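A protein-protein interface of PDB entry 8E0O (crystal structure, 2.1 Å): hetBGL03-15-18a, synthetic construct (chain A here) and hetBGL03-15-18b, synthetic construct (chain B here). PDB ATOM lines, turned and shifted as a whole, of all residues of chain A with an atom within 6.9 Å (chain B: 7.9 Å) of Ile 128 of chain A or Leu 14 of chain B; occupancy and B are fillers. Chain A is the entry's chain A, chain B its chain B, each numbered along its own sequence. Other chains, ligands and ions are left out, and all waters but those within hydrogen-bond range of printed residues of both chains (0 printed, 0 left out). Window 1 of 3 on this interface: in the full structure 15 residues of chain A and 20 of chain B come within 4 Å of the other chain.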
ATOM      1  N   LEU A 101      -3.185   4.314   9.786  1.00  0.00           N
ATOM      2  CA  LEU A 101      -3.296   3.939   8.380  1.00  0.00           C
ATOM      3  C   LEU A 101      -4.346   2.852   8.180  1.00  0.00           C
ATOM      4  O   LEU A 101      -5.106   2.883   7.205  1.00  0.00           O
ATOM      5  CB  LEU A 101      -1.936   3.472   7.860  1.00  0.00           C
ATOM      6  CG  LEU A 101      -1.816   3.142   6.371  1.00  0.00           C
ATOM      7  CD1 LEU A 101      -2.355   4.281   5.526  1.00  0.00           C
ATOM      8  CD2 LEU A 101      -0.372   2.833   6.004  1.00  0.00           C
ATOM      9  N   VAL A 104      -7.905   4.435   8.607  1.00  0.00           N
ATOM     10  CA  VAL A 104      -8.280   5.258   7.461  1.00  0.00           C
ATOM     11  C   VAL A 104      -8.641   4.379   6.271  1.00  0.00           C
ATOM     12  O   VAL A 104      -9.577   4.679   5.520  1.00  0.00           O
ATOM     13  CB  VAL A 104      -7.153   6.250   7.119  1.00  0.00           C
ATOM     14  CG1 VAL A 104      -7.504   7.048   5.870  1.00  0.00           C
ATOM     15  CG2 VAL A 104      -6.899   7.186   8.286  1.00  0.00           C
ATOM     16  N   ALA A 123     -10.693  10.866   2.807  1.00  0.00           N
ATOM     17  CA  ALA A 123     -10.033   9.687   3.358  1.00  0.00           C
ATOM     18  C   ALA A 123      -8.840   9.272   2.508  1.00  0.00           C
ATOM     19  O   ALA A 123      -7.797   8.881   3.045  1.00  0.00           O
ATOM     20  CB  ALA A 123     -11.032   8.536   3.482  1.00  0.00           C
ATOM     21  N   ASN A 124      -8.973   9.350   1.182  1.00  0.00           N
ATOM     22  CA  ASN A 124      -7.857   9.003   0.307  1.00  0.00           C
ATOM     23  C   ASN A 124      -6.706   9.988   0.465  1.00  0.00           C
ATOM     24  O   ASN A 124      -5.535   9.592   0.440  1.00  0.00           O
ATOM     25  CB  ASN A 124      -8.326   8.951  -1.146  1.00  0.00           C
ATOM     26  CG  ASN A 124      -7.198   8.648  -2.114  1.00  0.00           C
ATOM     27  OD1 ASN A 124      -6.781   9.510  -2.889  1.00  0.00           O
ATOM     28  ND2 ASN A 124      -6.699   7.418  -2.076  1.00  0.00           N
ATOM     29  N   ARG A 125      -7.019  11.277   0.627  1.00  0.00           N
ATOM     30  CA  ARG A 125      -5.974  12.267   0.866  1.00  0.00           C
ATOM     31  C   ARG A 125      -5.224  11.973   2.160  1.00  0.00           C
ATOM     32  O   ARG A 125      -3.990  12.038   2.200  1.00  0.00           O
ATOM     33  CB  ARG A 125      -6.580  13.670   0.903  1.00  0.00           C
ATOM     34  CG  ARG A 125      -5.593  14.774   1.259  1.00  0.00           C
ATOM     35  CD  ARG A 125      -4.461  14.867   0.245  1.00  0.00           C
ATOM     36  NE  ARG A 125      -3.625  16.041   0.466  1.00  0.00           N
ATOM     37  CZ  ARG A 125      -2.375  16.162   0.040  1.00  0.00           C
ATOM     38  N   LEU A 126      -5.955  11.639   3.227  1.00  0.00           N
ATOM     39  CA  LEU A 126      -5.303  11.265   4.477  1.00  0.00           C
ATOM     40  C   LEU A 126      -4.549   9.950   4.341  1.00  0.00           C
ATOM     41  O   LEU A 126      -3.498   9.773   4.968  1.00  0.00           O
ATOM     42  CB  LEU A 126      -6.338  11.176   5.601  1.00  0.00           C
ATOM     43  CG  LEU A 126      -5.811  10.825   6.993  1.00  0.00           C
ATOM     44  CD1 LEU A 126      -4.700  11.781   7.408  1.00  0.00           C
ATOM     45  CD2 LEU A 126      -6.939  10.836   8.014  1.00  0.00           C
ATOM     46  N   LEU A 127      -5.064   9.023   3.528  1.00  0.00           N
ATOM     47  CA  LEU A 127      -4.359   7.768   3.285  1.00  0.00           C
ATOM     48  C   LEU A 127      -2.993   8.018   2.657  1.00  0.00           C
ATOM     49  O   LEU A 127      -2.003   7.377   3.030  1.00  0.00           O
ATOM     50  CB  LEU A 127      -5.203   6.862   2.389  1.00  0.00           C
ATOM     51  CG  LEU A 127      -4.991   5.352   2.505  1.00  0.00           C
ATOM     52  CD1 LEU A 127      -5.483   4.836   3.847  1.00  0.00           C
ATOM     53  CD2 LEU A 127      -5.686   4.628   1.365  1.00  0.00           C
ATOM     54  N   ILE A 128      -2.924   8.943   1.700  1.00  0.00           N
ATOM     55  CA  ILE A 128      -1.646   9.295   1.088  1.00  0.00           C
ATOM     56  C   ILE A 128      -0.729   9.947   2.114  1.00  0.00           C
ATOM     57  O   ILE A 128       0.454   9.603   2.224  1.00  0.00           O
ATOM     58  CB  ILE A 128      -1.869  10.211  -0.130  1.00  0.00           C
ATOM     59  CG1 ILE A 128      -2.719   9.503  -1.186  1.00  0.00           C
ATOM     60  CG2 ILE A 128      -0.540  10.658  -0.718  1.00  0.00           C
ATOM     61  CD1 ILE A 128      -3.301  10.439  -2.227  1.00  0.00           C
ATOM     62  N   ASP A 129      -1.264  10.898   2.886  1.00  0.00           N
ATOM     63  CA  ASP A 129      -0.456  11.584   3.889  1.00  0.00           C
ATOM     64  C   ASP A 129       0.005  10.636   4.990  1.00  0.00           C
ATOM     65  O   ASP A 129       1.105  10.802   5.528  1.00  0.00           O
ATOM     66  CB  ASP A 129      -1.243  12.745   4.494  1.00  0.00           C
ATOM     67  CG  ASP A 129      -1.561  13.826   3.481  1.00  0.00           C
ATOM     68  OD1 ASP A 129      -0.825  13.940   2.478  1.00  0.00           O
ATOM     69  OD2 ASP A 129      -2.546  14.566   3.691  1.00  0.00           O
ATOM     70  N   ALA A 130      -0.814   9.639   5.335  1.00  0.00           N
ATOM     71  CA  ALA A 130      -0.438   8.706   6.391  1.00  0.00           C
ATOM     72  C   ALA A 130       0.676   7.772   5.934  1.00  0.00           C
ATOM     73  O   ALA A 130       1.560   7.422   6.725  1.00  0.00           O
ATOM     74  CB  ALA A 130      -1.657   7.908   6.850  1.00  0.00           C
ATOM     75  N   LEU A 131       0.651   7.352   4.666  1.00  0.00           N
ATOM     76  CA  LEU A 131       1.717   6.489   4.168  1.00  0.00           C
ATOM     77  C   LEU A 131       3.037   7.243   4.079  1.00  0.00           C
ATOM     78  O   LEU A 131       4.101   6.678   4.358  1.00  0.00           O
ATOM     79  CB  LEU A 131       1.344   5.904   2.805  1.00  0.00           C
ATOM     80  CG  LEU A 131       2.413   4.976   2.219  1.00  0.00           C
ATOM     81  CD1 LEU A 131       2.742   3.860   3.200  1.00  0.00           C
ATOM     82  CD2 LEU A 131       1.992   4.397   0.881  1.00  0.00           C
ATOM     83  N   GLU A 132       2.987   8.520   3.691  1.00  0.00           N
ATOM     84  CA  GLU A 132       4.201   9.330   3.665  1.00  0.00           C
ATOM     85  C   GLU A 132       4.824   9.423   5.050  1.00  0.00           C
ATOM     86  O   GLU A 132       6.052   9.362   5.194  1.00  0.00           O
ATOM     87  CB  GLU A 132       3.891  10.725   3.122  1.00  0.00           C
ATOM     88  CG  GLU A 132       5.089  11.660   3.100  1.00  0.00           C
ATOM     89  CD  GLU A 132       4.726  13.056   2.639  1.00  0.00           C
ATOM     90  OE1 GLU A 132       3.676  13.572   3.076  1.00  0.00           O
ATOM     91  OE2 GLU A 132       5.490  13.638   1.841  1.00  0.00           O
ATOM     92  N   VAL A 133       3.994   9.562   6.085  1.00  0.00           N
ATOM     93  CA  VAL A 133       4.507   9.614   7.449  1.00  0.00           C
ATOM     94  C   VAL A 133       5.089   8.264   7.848  1.00  0.00           C
ATOM     95  O   VAL A 133       6.189   8.186   8.409  1.00  0.00           O
ATOM     96  CB  VAL A 133       3.400  10.066   8.419  1.00  0.00           C
ATOM     97  CG1 VAL A 133       3.755   9.692   9.851  1.00  0.00           C
ATOM     98  CG2 VAL A 133       3.167  11.565   8.295  1.00  0.00           C
ATOM     99  N   ILE B   7       8.374  -1.222   1.996  1.00  0.00           N
ATOM    100  CA  ILE B   7       7.948   0.114   1.591  1.00  0.00           C
ATOM    101  C   ILE B   7       7.352   0.082   0.189  1.00  0.00           C
ATOM    102  O   ILE B   7       6.327   0.720  -0.079  1.00  0.00           O
ATOM    103  CB  ILE B   7       9.127   1.100   1.689  1.00  0.00           C
ATOM    104  CG1 ILE B   7       9.487   1.357   3.154  1.00  0.00           C
ATOM    105  CG2 ILE B   7       8.798   2.410   0.986  1.00  0.00           C
ATOM    106  CD1 ILE B   7      10.716   2.218   3.340  1.00  0.00           C
ATOM    107  N   GLU B   8       7.978  -0.665  -0.725  1.00  0.00           N
ATOM    108  CA  GLU B   8       7.435  -0.789  -2.074  1.00  0.00           C
ATOM    109  C   GLU B   8       6.086  -1.496  -2.069  1.00  0.00           C
ATOM    110  O   GLU B   8       5.219  -1.185  -2.894  1.00  0.00           O
ATOM    111  CB  GLU B   8       8.423  -1.532  -2.973  1.00  0.00           C
ATOM    112  N   GLU B   9       5.888  -2.444  -1.151  1.00  0.00           N
ATOM    113  CA  GLU B   9       4.593  -3.109  -1.044  1.00  0.00           C
ATOM    114  C   GLU B   9       3.528  -2.155  -0.516  1.00  0.00           C
ATOM    115  O   GLU B   9       2.367  -2.214  -0.938  1.00  0.00           O
ATOM    116  CB  GLU B   9       4.713  -4.344  -0.150  1.00  0.00           C
ATOM    117  CG  GLU B   9       3.390  -4.892   0.360  1.00  0.00           C
ATOM    118  CD  GLU B   9       3.441  -6.385   0.621  1.00  0.00           C
ATOM    119  OE1 GLU B   9       4.382  -6.842   1.305  1.00  0.00           O
ATOM    120  OE2 GLU B   9       2.539  -7.104   0.140  1.00  0.00           O
ATOM    121  N   LEU B  10       3.908  -1.258   0.399  1.00  0.00           N
ATOM    122  CA  LEU B  10       2.957  -0.281   0.919  1.00  0.00           C
ATOM    123  C   LEU B  10       2.564   0.733  -0.149  1.00  0.00           C
ATOM    124  O   LEU B  10       1.385   1.086  -0.272  1.00  0.00           O
ATOM    125  CB  LEU B  10       3.548   0.429   2.137  1.00  0.00           C
ATOM    126  CG  LEU B  10       3.547  -0.337   3.461  1.00  0.00           C
ATOM    127  CD1 LEU B  10       4.464   0.340   4.467  1.00  0.00           C
ATOM    128  CD2 LEU B  10       2.136  -0.450   4.014  1.00  0.00           C
ATOM    129  N   VAL B  11       3.536   1.214  -0.927  1.00  0.00           N
ATOM    130  CA  VAL B  11       3.235   2.177  -1.982  1.00  0.00           C
ATOM    131  C   VAL B  11       2.388   1.529  -3.071  1.00  0.00           C
ATOM    132  O   VAL B  11       1.471   2.154  -3.617  1.00  0.00           O
ATOM    133  CB  VAL B  11       4.539   2.768  -2.550  1.00  0.00           C
ATOM    134  CG1 VAL B  11       4.245   3.693  -3.723  1.00  0.00           C
ATOM    135  CG2 VAL B  11       5.299   3.512  -1.461  1.00  0.00           C
ATOM    136  N   LYS B  12       2.676   0.267  -3.399  1.00  0.00           N
ATOM    137  CA  LYS B  12       1.868  -0.440  -4.387  1.00  0.00           C
ATOM    138  C   LYS B  12       0.434  -0.624  -3.907  1.00  0.00           C
ATOM    139  O   LYS B  12      -0.497  -0.619  -4.719  1.00  0.00           O
ATOM    140  CB  LYS B  12       2.499  -1.794  -4.711  1.00  0.00           C
ATOM    141  CG  LYS B  12       3.458  -1.767  -5.892  1.00  0.00           C
ATOM    142  CD  LYS B  12       3.899  -3.171  -6.277  1.00  0.00           C
ATOM    143  CE  LYS B  12       4.847  -3.149  -7.467  1.00  0.00           C
ATOM    144  NZ  LYS B  12       4.908  -1.808  -8.113  1.00  0.00           N
ATOM    145  N   GLU B  13       0.237  -0.786  -2.596  1.00  0.00           N
ATOM    146  CA  GLU B  13      -1.115  -0.913  -2.065  1.00  0.00           C
ATOM    147  C   GLU B  13      -1.861   0.415  -2.130  1.00  0.00           C
ATOM    148  O   GLU B  13      -3.061   0.445  -2.426  1.00  0.00           O
ATOM    149  CB  GLU B  13      -1.071  -1.437  -0.630  1.00  0.00           C
ATOM    150  N   LEU B  14      -1.168   1.523  -1.855  1.00  0.00           N
ATOM    151  CA  LEU B  14      -1.808   2.831  -1.949  1.00  0.00           C
ATOM    152  C   LEU B  14      -2.183   3.156  -3.390  1.00  0.00           C
ATOM    153  O   LEU B  14      -3.212   3.794  -3.643  1.00  0.00           O
ATOM    154  CB  LEU B  14      -0.892   3.912  -1.372  1.00  0.00           C
ATOM    155  CG  LEU B  14      -1.428   5.345  -1.421  1.00  0.00           C
ATOM    156  CD1 LEU B  14      -2.747   5.447  -0.673  1.00  0.00           C
ATOM    157  CD2 LEU B  14      -0.419   6.332  -0.855  1.00  0.00           C
ATOM    158  N   ILE B  15      -1.360   2.721  -4.347  1.00  0.00           N
ATOM    159  CA  ILE B  15      -1.673   2.938  -5.758  1.00  0.00           C
ATOM    160  C   ILE B  15      -2.948   2.194  -6.134  1.00  0.00           C
ATOM    161  O   ILE B  15      -3.853   2.752  -6.766  1.00  0.00           O
ATOM    162  CB  ILE B  15      -0.489   2.507  -6.640  1.00  0.00           C
ATOM    163  CG1 ILE B  15       0.623   3.555  -6.598  1.00  0.00           C
ATOM    164  CG2 ILE B  15      -0.943   2.284  -8.075  1.00  0.00           C
ATOM    165  CD1 ILE B  15       1.932   3.072  -7.186  1.00  0.00           C
ATOM    166  N   LYS B  16      -3.036   0.918  -5.747  1.00  0.00           N
ATOM    167  CA  LYS B  16      -4.220   0.125  -6.064  1.00  0.00           C
ATOM    168  C   LYS B  16      -5.463   0.686  -5.373  1.00  0.00           C
ATOM    169  O   LYS B  16      -6.558   0.658  -5.944  1.00  0.00           O
ATOM    170  CB  LYS B  16      -3.998  -1.334  -5.665  1.00  0.00           C
ATOM    171  N   HIS B  17      -5.302   1.187  -4.149  1.00  0.00           N
ATOM    172  CA  HIS B  17      -6.426   1.793  -3.441  1.00  0.00           C
ATOM    173  C   HIS B  17      -6.900   3.060  -4.141  1.00  0.00           C
ATOM    174  O   HIS B  17      -8.108   3.276  -4.298  1.00  0.00           O
ATOM    175  CB  HIS B  17      -6.033   2.102  -1.996  1.00  0.00           C
ATOM    176  CG  HIS B  17      -6.095   0.919  -1.081  1.00  0.00           C
ATOM    177  ND1 HIS B  17      -4.976   0.380  -0.484  1.00  0.00           N
ATOM    178  CD2 HIS B  17      -7.144   0.174  -0.656  1.00  0.00           C
ATOM    179  CE1 HIS B  17      -5.331  -0.647   0.267  1.00  0.00           C
ATOM    180  NE2 HIS B  17      -6.642  -0.793   0.180  1.00  0.00           N
ATOM    181  N   THR B  18      -5.962   3.909  -4.566  1.00  0.00           N
ATOM    182  CA  THR B  18      -6.331   5.150  -5.237  1.00  0.00           C
ATOM    183  C   THR B  18      -6.922   4.875  -6.616  1.00  0.00           C
ATOM    184  O   THR B  18      -7.860   5.558  -7.044  1.00  0.00           O
ATOM    185  CB  THR B  18      -5.113   6.069  -5.342  1.00  0.00           C
ATOM    186  OG1 THR B  18      -4.590   6.318  -4.031  1.00  0.00           O
ATOM    187  CG2 THR B  18      -5.494   7.396  -5.983  1.00  0.00           C
ATOM    188  N   GLU B  19      -6.390   3.873  -7.322  1.00  0.00           N
ATOM    189  CA  GLU B  19      -6.958   3.500  -8.613  1.00  0.00           C
ATOM    190  C   GLU B  19      -8.380   2.976  -8.464  1.00  0.00           C
ATOM    191  O   GLU B  19      -9.204   3.151  -9.370  1.00  0.00           O
ATOM    192  CB  GLU B  19      -6.074   2.457  -9.297  1.00  0.00           C
ATOM    193  N   GLU B  20      -8.687   2.331  -7.336  1.00  0.00           N
ATOM    194  CA  GLU B  20     -10.059   1.908  -7.079  1.00  0.00           C
ATOM    195  C   GLU B  20     -10.981   3.112  -6.926  1.00  0.00           C
ATOM    196  O   GLU B  20     -12.120   3.096  -7.407  1.00  0.00           O
ATOM    197  CB  GLU B  20     -10.113   1.026  -5.831  1.00  0.00           C
ATOM    198  N   LEU B  21     -10.504   4.166  -6.260  1.00  0.00           N
ATOM    199  CA  LEU B  21     -11.289   5.393  -6.165  1.00  0.00           C
ATOM    200  C   LEU B  21     -11.468   6.034  -7.535  1.00  0.00           C
ATOM    201  O   LEU B  21     -12.532   6.585  -7.839  1.00  0.00           O
ATOM    202  CB  LEU B  21     -10.623   6.371  -5.198  1.00  0.00           C
ATOM    203  CG  LEU B  21     -11.392   7.666  -4.927  1.00  0.00           C
ATOM    204  CD1 LEU B  21     -12.794   7.362  -4.419  1.00  0.00           C
ATOM    205  CD2 LEU B  21     -10.639   8.548  -3.943  1.00  0.00           C
ATOM    206  N   GLU B  41     -10.739  17.444  -7.102  1.00  0.00           N
ATOM    207  CA  GLU B  41     -10.166  16.978  -5.845  1.00  0.00           C
ATOM    208  C   GLU B  41      -9.443  15.650  -6.024  1.00  0.00           C
ATOM    209  O   GLU B  41      -8.408  15.411  -5.392  1.00  0.00           O
ATOM    210  CB  GLU B  41     -11.253  16.856  -4.781  1.00  0.00           C
ATOM    211  CG  GLU B  41     -10.703  16.586  -3.398  1.00  0.00           C
ATOM    212  CD  GLU B  41     -11.749  16.711  -2.317  1.00  0.00           C
ATOM    213  OE1 GLU B  41     -12.905  17.061  -2.638  1.00  0.00           O
ATOM    214  OE2 GLU B  41     -11.410  16.458  -1.144  1.00  0.00           O
ATOM    215  N   LEU B  42      -9.975  14.770  -6.876  1.00  0.00           N
ATOM    216  CA  LEU B  42      -9.281  13.520  -7.166  1.00  0.00           C
ATOM    217  C   LEU B  42      -7.957  13.783  -7.872  1.00  0.00           C
ATOM    218  O   LEU B  42      -6.950  13.124  -7.586  1.00  0.00           O
ATOM    219  CB  LEU B  42     -10.171  12.607  -8.010  1.00  0.00           C
ATOM    220  CG  LEU B  42      -9.517  11.344  -8.576  1.00  0.00           C
ATOM    221  CD1 LEU B  42      -8.972  10.470  -7.453  1.00  0.00           C
ATOM    222  CD2 LEU B  42     -10.502  10.569  -9.435  1.00  0.00           C
ATOM    223  N   GLU B  44      -6.172  16.413  -7.455  1.00  0.00           N
ATOM    224  CA  GLU B  44      -5.279  16.918  -6.416  1.00  0.00           C
ATOM    225  C   GLU B  44      -4.669  15.774  -5.618  1.00  0.00           C
ATOM    226  O   GLU B  44      -3.486  15.817  -5.261  1.00  0.00           O
ATOM    227  CB  GLU B  44      -6.033  17.877  -5.495  1.00  0.00           C
ATOM    228  N   ASN B  45      -5.462  14.738  -5.332  1.00  0.00           N
ATOM    229  CA  ASN B  45      -4.929  13.570  -4.637  1.00  0.00           C
ATOM    230  C   ASN B  45      -3.901  12.839  -5.493  1.00  0.00           C
ATOM    231  O   ASN B  45      -2.899  12.334  -4.973  1.00  0.00           O
ATOM    232  CB  ASN B  45      -6.066  12.624  -4.246  1.00  0.00           C
ATOM    233  CG  ASN B  45      -6.949  13.190  -3.149  1.00  0.00           C
ATOM    234  OD1 ASN B  45      -6.803  14.345  -2.750  1.00  0.00           O
ATOM    235  ND2 ASN B  45      -7.873  12.374  -2.656  1.00  0.00           N
ATOM    236  N   LEU B  46      -4.133  12.773  -6.808  1.00  0.00           N
ATOM    237  CA  LEU B  46      -3.193  12.088  -7.690  1.00  0.00           C
ATOM    238  C   LEU B  46      -1.841  12.789  -7.708  1.00  0.00           C
ATOM    239  O   LEU B  46      -0.793  12.134  -7.739  1.00  0.00           O
ATOM    240  CB  LEU B  46      -3.769  11.995  -9.104  1.00  0.00           C
ATOM    241  CG  LEU B  46      -5.004  11.109  -9.281  1.00  0.00           C
ATOM    242  CD1 LEU B  46      -5.474  11.119 -10.727  1.00  0.00           C
ATOM    243  CD2 LEU B  46      -4.719   9.690  -8.817  1.00  0.00           C
ATOM    244  N   VAL B  47      -1.844  14.124  -7.693  1.00  0.00           N
ATOM    245  CA  VAL B  47      -0.589  14.866  -7.632  1.00  0.00           C
ATOM    246  C   VAL B  47       0.106  14.626  -6.298  1.00  0.00           C
ATOM    247  O   VAL B  47       1.327  14.438  -6.242  1.00  0.00           O
ATOM    248  CB  VAL B  47      -0.842  16.364  -7.881  1.00  0.00           C
ATOM    249  CG1 VAL B  47       0.442  17.160  -7.697  1.00  0.00           C
ATOM    250  CG2 VAL B  47      -1.415  16.581  -9.271  1.00  0.00           C
ATOM    251  N   ARG B  48      -0.660  14.627  -5.203  1.00  0.00           N
ATOM    252  CA  ARG B  48      -0.081  14.325  -3.898  1.00  0.00           C
ATOM    253  C   ARG B  48       0.446  12.897  -3.851  1.00  0.00           C
ATOM    254  O   ARG B  48       1.505  12.636  -3.268  1.00  0.00           O
ATOM    255  CB  ARG B  48      -1.119  14.553  -2.798  1.00  0.00           C
ATOM    256  N   LEU B  49      -0.280  11.958  -4.462  1.00  0.00           N
ATOM    257  CA  LEU B  49       0.196  10.580  -4.525  1.00  0.00           C
ATOM    258  C   LEU B  49       1.467  10.477  -5.358  1.00  0.00           C
ATOM    259  O   LEU B  49       2.412   9.775  -4.979  1.00  0.00           O
ATOM    260  CB  LEU B  49      -0.895   9.674  -5.094  1.00  0.00           C
ATOM    261  CG  LEU B  49      -0.504   8.229  -5.416  1.00  0.00           C
ATOM    262  CD1 LEU B  49       0.118   7.544  -4.207  1.00  0.00           C
ATOM    263  CD2 LEU B  49      -1.703   7.443  -5.922  1.00  0.00           C
ATOM    264  N   ALA B  50       1.508  11.172  -6.499  1.00  0.00           N
ATOM    265  CA  ALA B  50       2.699  11.142  -7.343  1.00  0.00           C
ATOM    266  C   ALA B  50       3.907  11.716  -6.616  1.00  0.00           C
ATOM    267  O   ALA B  50       5.036  11.249  -6.806  1.00  0.00           O
ATOM    268  CB  ALA B  50       2.441  11.905  -8.642  1.00  0.00           C
ATOM    269  N   ARG B  51       3.688  12.736  -5.779  1.00  0.00           N
ATOM    270  CA  ARG B  51       4.781  13.297  -4.989  1.00  0.00           C
ATOM    271  C   ARG B  51       5.331  12.274  -4.002  1.00  0.00           C
ATOM    272  O   ARG B  51       6.552  12.139  -3.851  1.00  0.00           O
ATOM    273  CB  ARG B  51       4.300  14.549  -4.250  1.00  0.00           C
ATOM    274  CG  ARG B  51       5.296  15.104  -3.233  1.00  0.00           C
ATOM    275  CD  ARG B  51       5.118  16.600  -2.987  1.00  0.00           C
ATOM    276  NE  ARG B  51       6.384  17.328  -2.992  1.00  0.00           N
ATOM    277  CZ  ARG B  51       6.756  18.206  -3.914  1.00  0.00           C
ATOM    278  NH1 ARG B  51       5.956  18.539  -4.916  1.00  0.00           N
ATOM    279  NH2 ARG B  51       7.952  18.784  -3.815  1.00  0.00           N
ATOM    280  N   VAL B  52       4.446  11.543  -3.320  1.00  0.00           N
ATOM    281  CA  VAL B  52       4.892  10.547  -2.350  1.00  0.00           C
ATOM    282  C   VAL B  52       5.571   9.380  -3.055  1.00  0.00           C
ATOM    283  O   VAL B  52       6.544   8.808  -2.546  1.00  0.00           O
ATOM    284  CB  VAL B  52       3.707  10.079  -1.484  1.00  0.00           C
ATOM    285  CG1 VAL B  52       4.132   8.959  -0.544  1.00  0.00           C
ATOM    286  CG2 VAL B  52       3.133  11.246  -0.697  1.00  0.00           C
ATOM    287  N   ILE B  53       5.079   9.012  -4.241  1.00  0.00           N
ATOM    288  CA  ILE B  53       5.664   7.897  -4.981  1.00  0.00           C
ATOM    289  C   ILE B  53       7.088   8.234  -5.402  1.00  0.00           C
ATOM    290  O   ILE B  53       8.015   7.434  -5.223  1.00  0.00           O
ATOM    291  CB  ILE B  53       4.789   7.545  -6.197  1.00  0.00           C
ATOM    292  CG1 ILE B  53       3.486   6.886  -5.753  1.00  0.00           C
ATOM    293  CG2 ILE B  53       5.535   6.606  -7.129  1.00  0.00           C
ATOM    294  CD1 ILE B  53       2.531   6.627  -6.894  1.00  0.00           C
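Hydrophobic or aromatic side chains of chain B that line the printed part of chain A: Leu 10, Leu 14, Leu 21, Leu 49 and Val 52.
Among the printed residues, 15 pairs touch across the chains.
Ile 128 of chain A touches just these residues of chain B: Leu 14, Asn 45, Arg 48, Leu 49 and Val 52.
Printed residues of chain B within 4 Å of Leu 131 of chain A: Leu 10 (3.6 Å), Val 11 (3.8 Å) and Leu 14 (3.5 Å).
Printed residues of chain A within 4 Å of Leu 10 of chain B: Leu 131.
Of the printed residues of chain A, Leu 14 of chain B touches Leu 127, Ile 128 and Leu 131.
Of the printed residues of chain A, Leu 21 of chain B touches Asn 124.
Printed residues of chain A within 4 Å of Asn 45 of chain B: Asn 124, Arg 125 and Ile 128.
The nearest residue of chain B that does not touch Ile 128 of chain A is Thr 18 of chain B (4.7 Å).
The nearest printed residue of chain B that does not touch Leu 131 of chain A is Val 52 of chain B (5.1 Å).
NE of Arg 125 of chain A is in salt-bridge range of OD2 of Asp 129 of chain A, 3.7 Å away.
The backbone carbonyl oxygen (O) of Leu 14 of chain B sits at hydrogen-bond distance from the side-chain hydroxyl (OG1) of Thr 18 of chain B (2.9 Å).
The backbone carbonyl oxygen (O) of Glu 41 of chain B sits close to the side-chain amide oxygen (OD1) of Asn 45 of chain B.
The side-chain hydroxyl (OG1) of Thr 18 of chain B lies within hydrogen-bond range of the side-chain amide nitrogen (ND2) of Asn 124 of chain A, 3.1 Å away.
The side-chain amide oxygen (OD1) of Asn 124 of chain A is in hydrogen-bond range of the side-chain amide nitrogen (ND2) of Asn 45 of chain B.
CB of Asn 124 of chain A touches CD2 of Leu 21 of chain B, at 3.7 Å.
Arg 125 of chain A touches Asn 45 of chain B (N to ND2, 3.6 Å).
Arg 125 of chain A touches Arg 48 of chain B (CZ to CB, 3.5 Å).
CD2 of Leu 127 of chain A touches CD1 of Leu 14 of chain B (3.7 Å).
Leu 14 of chain B touches Ile 128 of chain A.
CD1 of Ile 128 of chain A touches O of Asn 45 of chain B, at 3.4 Å.
Ile 128 of chain A touches Leu 49 of chain B (CD1 to CB, 3.8 Å).
Ile 128 of chain A touches Val 52 of chain B (CG2 to CG2, 3.7 Å).
CD2 of Leu 131 of chain A touches CA of Val 11 of chain B, at 3.8 Å.
Leu 131 of chain A touches Leu 14 of chain B.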
